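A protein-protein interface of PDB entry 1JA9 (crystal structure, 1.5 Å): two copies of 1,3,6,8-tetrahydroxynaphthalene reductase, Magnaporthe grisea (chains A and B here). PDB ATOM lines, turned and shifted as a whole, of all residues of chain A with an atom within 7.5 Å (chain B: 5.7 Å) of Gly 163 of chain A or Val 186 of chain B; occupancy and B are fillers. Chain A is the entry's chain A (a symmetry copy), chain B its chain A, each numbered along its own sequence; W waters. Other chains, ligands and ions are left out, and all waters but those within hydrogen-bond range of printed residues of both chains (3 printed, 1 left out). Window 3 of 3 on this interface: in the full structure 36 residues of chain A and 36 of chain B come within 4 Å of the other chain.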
ATOM      1  N   VAL A 160      -4.016  17.153   7.352  1.00  0.00           N
ATOM      2  CA  VAL A 160      -5.071  18.150   7.205  1.00  0.00           C
ATOM      3  C   VAL A 160      -5.067  19.221   8.281  1.00  0.00           C
ATOM      4  O   VAL A 160      -5.922  20.103   8.263  1.00  0.00           O
ATOM      5  CB  VAL A 160      -6.493  17.474   7.148  1.00  0.00           C
ATOM      6  CG1 VAL A 160      -6.589  16.585   5.943  1.00  0.00           C
ATOM      7  CG2 VAL A 160      -6.755  16.666   8.415  1.00  0.00           C
ATOM      8  N   MET A 161      -4.114  19.169   9.199  1.00  0.00           N
ATOM      9  CA  MET A 161      -4.070  20.168  10.272  1.00  0.00           C
ATOM     10  C   MET A 161      -3.581  21.517   9.773  1.00  0.00           C
ATOM     11  O   MET A 161      -2.883  21.612   8.767  1.00  0.00           O
ATOM     12  CB  MET A 161      -3.135  19.757  11.396  1.00  0.00           C
ATOM     13  CG  MET A 161      -3.728  18.802  12.366  1.00  0.00           C
ATOM     14  SD  MET A 161      -2.408  18.353  13.546  1.00  0.00           S
ATOM     15  CE  MET A 161      -2.546  19.852  14.606  1.00  0.00           C
ATOM     16  N   THR A 162      -3.946  22.564  10.497  1.00  0.00           N
ATOM     17  CA  THR A 162      -3.510  23.895  10.144  1.00  0.00           C
ATOM     18  C   THR A 162      -2.692  24.396  11.339  1.00  0.00           C
ATOM     19  O   THR A 162      -2.695  23.772  12.406  1.00  0.00           O
ATOM     20  CB  THR A 162      -4.730  24.804   9.887  1.00  0.00           C
ATOM     21  OG1 THR A 162      -5.553  24.837  11.063  1.00  0.00           O
ATOM     22  CG2 THR A 162      -5.549  24.259   8.731  1.00  0.00           C
ATOM     23  N   GLY A 163      -1.915  25.450  11.126  1.00  0.00           N
ATOM     24  CA  GLY A 163      -1.144  26.034  12.211  1.00  0.00           C
ATOM     25  C   GLY A 163       0.151  25.368  12.641  1.00  0.00           C
ATOM     26  O   GLY A 163       0.731  25.767  13.653  1.00  0.00           O
ATOM     27  N   ILE A 164       0.606  24.359  11.904  1.00  0.00           N
ATOM     28  CA  ILE A 164       1.845  23.667  12.243  1.00  0.00           C
ATOM     29  C   ILE A 164       2.924  24.132  11.271  1.00  0.00           C
ATOM     30  O   ILE A 164       2.746  24.043  10.039  1.00  0.00           O
ATOM     31  CB  ILE A 164       1.682  22.137  12.103  1.00  0.00           C
ATOM     32  CG1 ILE A 164       0.558  21.630  13.012  1.00  0.00           C
ATOM     33  CG2 ILE A 164       2.975  21.453  12.503  1.00  0.00           C
ATOM     34  CD1 ILE A 164       0.848  21.748  14.489  1.00  0.00           C
ATOM     35  N   PRO A 165       4.042  24.670  11.797  1.00  0.00           N
ATOM     36  CA  PRO A 165       5.156  25.157  10.971  1.00  0.00           C
ATOM     37  C   PRO A 165       6.238  24.111  10.653  1.00  0.00           C
ATOM     38  O   PRO A 165       6.348  23.089  11.350  1.00  0.00           O
ATOM     39  CB  PRO A 165       5.764  26.255  11.857  1.00  0.00           C
ATOM     40  CG  PRO A 165       5.660  25.641  13.217  1.00  0.00           C
ATOM     41  CD  PRO A 165       4.259  24.996  13.226  1.00  0.00           C
ATOM     42  N   ASN A 166       7.033  24.398   9.612  1.00  0.00           N
ATOM     43  CA  ASN A 166       8.182  23.566   9.203  1.00  0.00           C
ATOM     44  C   ASN A 166       7.811  22.089   8.978  1.00  0.00           C
ATOM     45  O   ASN A 166       8.652  21.182   9.158  1.00  0.00           O
ATOM     46  CB  ASN A 166       9.244  23.648  10.308  1.00  0.00           C
ATOM     47  CG  ASN A 166       9.540  25.089  10.710  1.00  0.00           C
ATOM     48  OD1 ASN A 166       9.390  25.471  11.878  1.00  0.00           O
ATOM     49  ND2 ASN A 166       9.885  25.901   9.733  1.00  0.00           N
ATOM     50  N   HIS A 167       6.612  21.872   8.445  1.00  0.00           N
ATOM     51  CA  HIS A 167       6.129  20.514   8.308  1.00  0.00           C
ATOM     52  C   HIS A 167       5.567  20.150   6.940  1.00  0.00           C
ATOM     53  O   HIS A 167       4.796  19.195   6.836  1.00  0.00           O
ATOM     54  CB  HIS A 167       5.032  20.329   9.362  1.00  0.00           C
ATOM     55  CG  HIS A 167       4.930  18.938   9.886  1.00  0.00           C
ATOM     56  ND1 HIS A 167       3.732  18.374  10.260  1.00  0.00           N
ATOM     57  CD2 HIS A 167       5.887  18.042  10.218  1.00  0.00           C
ATOM     58  CE1 HIS A 167       3.952  17.194  10.806  1.00  0.00           C
ATOM     59  NE2 HIS A 167       5.253  16.968  10.797  1.00  0.00           N
ATOM     60  N   HIS A 214       5.599  19.316  19.366  1.00  0.00           N
ATOM     61  CA  HIS A 214       5.151  20.145  18.242  1.00  0.00           C
ATOM     62  C   HIS A 214       3.625  20.246  18.158  1.00  0.00           C
ATOM     63  O   HIS A 214       3.089  21.172  17.546  1.00  0.00           O
ATOM     64  CB  HIS A 214       5.612  19.566  16.908  1.00  0.00           C
ATOM     65  CG  HIS A 214       7.089  19.572  16.692  1.00  0.00           C
ATOM     66  ND1 HIS A 214       7.746  20.621  16.095  1.00  0.00           N
ATOM     67  CD2 HIS A 214       8.015  18.601  16.859  1.00  0.00           C
ATOM     68  CE1 HIS A 214       9.005  20.298  15.884  1.00  0.00           C
ATOM     69  NE2 HIS A 214       9.196  19.076  16.338  1.00  0.00           N
ATOM     70  N   CYS B 181       0.086  23.235   0.764  1.00  0.00           N
ATOM     71  CA  CYS B 181      -0.594  24.508   0.890  1.00  0.00           C
ATOM     72  C   CYS B 181      -0.829  24.909   2.349  1.00  0.00           C
ATOM     73  O   CYS B 181      -0.496  26.036   2.767  1.00  0.00           O
ATOM     74  CB  CYS B 181      -1.907  24.433   0.122  1.00  0.00           C
ATOM     75  SG  CYS B 181      -3.047  25.792   0.469  1.00  0.00           S
ATOM     76  N   ARG B 182      -1.361  23.994   3.150  1.00  0.00           N
ATOM     77  CA  ARG B 182      -1.620  24.317   4.552  1.00  0.00           C
ATOM     78  C   ARG B 182      -0.340  24.603   5.322  1.00  0.00           C
ATOM     79  O   ARG B 182      -0.327  25.446   6.213  1.00  0.00           O
ATOM     80  CB  ARG B 182      -2.381  23.165   5.222  1.00  0.00           C
ATOM     81  CG  ARG B 182      -3.783  23.015   4.661  1.00  0.00           C
ATOM     82  CD  ARG B 182      -4.552  21.906   5.348  1.00  0.00           C
ATOM     83  NE  ARG B 182      -4.291  20.599   4.769  1.00  0.00           N
ATOM     84  CZ  ARG B 182      -4.922  20.122   3.706  1.00  0.00           C
ATOM     85  NH1 ARG B 182      -5.838  20.850   3.103  1.00  0.00           N
ATOM     86  NH2 ARG B 182      -4.669  18.899   3.282  1.00  0.00           N
ATOM     87  N   ALA B 183       0.708  23.838   5.018  1.00  0.00           N
ATOM     88  CA  ALA B 183       2.008  23.973   5.680  1.00  0.00           C
ATOM     89  C   ALA B 183       2.686  25.287   5.312  1.00  0.00           C
ATOM     90  O   ALA B 183       3.097  26.062   6.178  1.00  0.00           O
ATOM     91  CB  ALA B 183       2.912  22.777   5.298  1.00  0.00           C
ATOM     92  N   PHE B 184       2.773  25.542   4.015  1.00  0.00           N
ATOM     93  CA  PHE B 184       3.395  26.766   3.549  1.00  0.00           C
ATOM     94  C   PHE B 184       2.656  28.015   4.003  1.00  0.00           C
ATOM     95  O   PHE B 184       3.278  29.040   4.191  1.00  0.00           O
ATOM     96  CB  PHE B 184       3.578  26.758   2.032  1.00  0.00           C
ATOM     97  CG  PHE B 184       4.895  26.173   1.604  1.00  0.00           C
ATOM     98  CD1 PHE B 184       5.004  24.815   1.324  1.00  0.00           C
ATOM     99  CD2 PHE B 184       6.045  26.981   1.485  1.00  0.00           C
ATOM    100  CE1 PHE B 184       6.235  24.258   0.926  1.00  0.00           C
ATOM    101  CE2 PHE B 184       7.281  26.425   1.083  1.00  0.00           C
ATOM    102  CZ  PHE B 184       7.367  25.071   0.804  1.00  0.00           C
ATOM    103  N   ALA B 185       1.336  27.950   4.179  1.00  0.00           N
ATOM    104  CA  ALA B 185       0.621  29.142   4.627  1.00  0.00           C
ATOM    105  C   ALA B 185       1.163  29.561   6.012  1.00  0.00           C
ATOM    106  O   ALA B 185       1.417  30.748   6.277  1.00  0.00           O
ATOM    107  CB  ALA B 185      -0.892  28.871   4.676  1.00  0.00           C
ATOM    108  N   VAL B 186       1.428  28.573   6.861  1.00  0.00           N
ATOM    109  CA  VAL B 186       1.954  28.863   8.192  1.00  0.00           C
ATOM    110  C   VAL B 186       3.373  29.404   8.041  1.00  0.00           C
ATOM    111  O   VAL B 186       3.710  30.422   8.627  1.00  0.00           O
ATOM    112  CB  VAL B 186       1.991  27.603   9.076  1.00  0.00           C
ATOM    113  CG1 VAL B 186       2.746  27.892  10.363  1.00  0.00           C
ATOM    114  CG2 VAL B 186       0.591  27.151   9.378  1.00  0.00           C
ATOM    115  N   ASP B 187       4.161  28.769   7.177  1.00  0.00           N
ATOM    116  CA  ASP B 187       5.558  29.151   6.958  1.00  0.00           C
ATOM    117  C   ASP B 187       5.808  30.504   6.286  1.00  0.00           C
ATOM    118  O   ASP B 187       6.870  31.095   6.450  1.00  0.00           O
ATOM    119  CB  ASP B 187       6.292  28.022   6.218  1.00  0.00           C
ATOM    120  CG  ASP B 187       6.300  26.730   7.033  1.00  0.00           C
ATOM    121  OD1 ASP B 187       6.091  25.653   6.446  1.00  0.00           O
ATOM    122  OD2 ASP B 187       6.475  26.804   8.271  1.00  0.00           O
ATOM    123  N   CYS B 188       4.824  30.980   5.539  1.00  0.00           N
ATOM    124  CA  CYS B 188       4.933  32.245   4.827  1.00  0.00           C
ATOM    125  C   CYS B 188       4.295  33.408   5.561  1.00  0.00           C
ATOM    126  O   CYS B 188       4.393  34.539   5.111  1.00  0.00           O
ATOM    127  CB  CYS B 188       4.261  32.120   3.452  1.00  0.00           C
ATOM    128  SG  CYS B 188       5.104  30.994   2.341  1.00  0.00           S
ATOM    129  N   GLY B 189       3.610  33.126   6.660  1.00  0.00           N
ATOM    130  CA  GLY B 189       2.921  34.168   7.406  1.00  0.00           C
ATOM    131  C   GLY B 189       3.759  35.363   7.832  1.00  0.00           C
ATOM    132  O   GLY B 189       3.335  36.523   7.660  1.00  0.00           O
ATOM    133  N   ALA B 190       4.912  35.094   8.442  1.00  0.00           N
ATOM    134  CA  ALA B 190       5.784  36.173   8.907  1.00  0.00           C
ATOM    135  C   ALA B 190       6.162  37.126   7.772  1.00  0.00           C
ATOM    136  O   ALA B 190       6.309  38.330   7.997  1.00  0.00           O
ATOM    137  CB  ALA B 190       7.018  35.602   9.540  1.00  0.00           C
HETATM  138  O   HOH W   1       9.496  26.834   7.058  1.00  0.00           O
HETATM  139  O   HOH W   2      -0.025  23.713   8.967  1.00  0.00           O
HETATM  140  O   HOH W   3      -1.955  19.963   6.791  1.00  0.00           O
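OD2 of Asp 187 of chain B lies within hydrogen-bond range of N of Asn 166 of chain A.
Among the printed residues, merely in contact across the chains: Val 160 of chain A with Arg 182 of chain B (3.5 Å), Met 161 of chain A with Arg 182 of chain B (3.8 Å), Gly 163 of chain A with Val 186 of chain B (3.5 Å), Ile 164 of chain A with Val 186 of chain B (3.8 Å), Pro 165 of chain A with Val 186 of chain B (3.7 Å) and Pro 165 of chain A with Asp 187 of chain B (3.4 Å).
Of the printed residues of chain B, Val 160 of chain A touches Arg 182. Gly 163 of chain A touches just one residue of chain B: Val 186 (3.5 Å). Printed residues of chain B within 4 Å of Ile 164 of chain A: Val 186. Of the printed residues of chain B, Pro 165 of chain A touches Val 186 (3.7 Å) and Asp 187 (3.4 Å). His 167 of chain A touches none of the printed residues of chain B. Of the printed residues of chain A, Arg 182 of chain B touches Val 160 (3.5 Å) and Met 161 (3.8 Å). Val 186 of chain B touches three residues of chain A. The nearest printed residue of chain B that does not touch Asn 166 of chain A is Ala 183 of chain B (5.5 Å).
Hydrophobic or aromatic side chains of chain A that line the printed part of chain B: Pro 165. Along chain A the printed residues that touch a printed residue of chain B span positions 160 to 166. Among the printed residues, 7 pairs touch across the chains.
No position is printed for both chains. Of the 7 pairs that touch across the chains among the printed residues, none has its exchanged pair printed and touching as well.
Water W3 bridges the backbone carbonyl oxygen of Met 161 of chain A (2.7 Å) and the guanidinium group of Arg 182 of chain B (3.2 Å). Water W1 bridges ND2 of Asn 166 of chain A (2.9 Å) and OD2 of Asp 187 of chain B (3.3 Å). Water W2 lies within hydrogen-bond range of O of Ile 164 of chain A (3.0 Å), O of Arg 182 of chain B (3.3 Å) and N of Gly 163 of chain A (3.4 Å).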
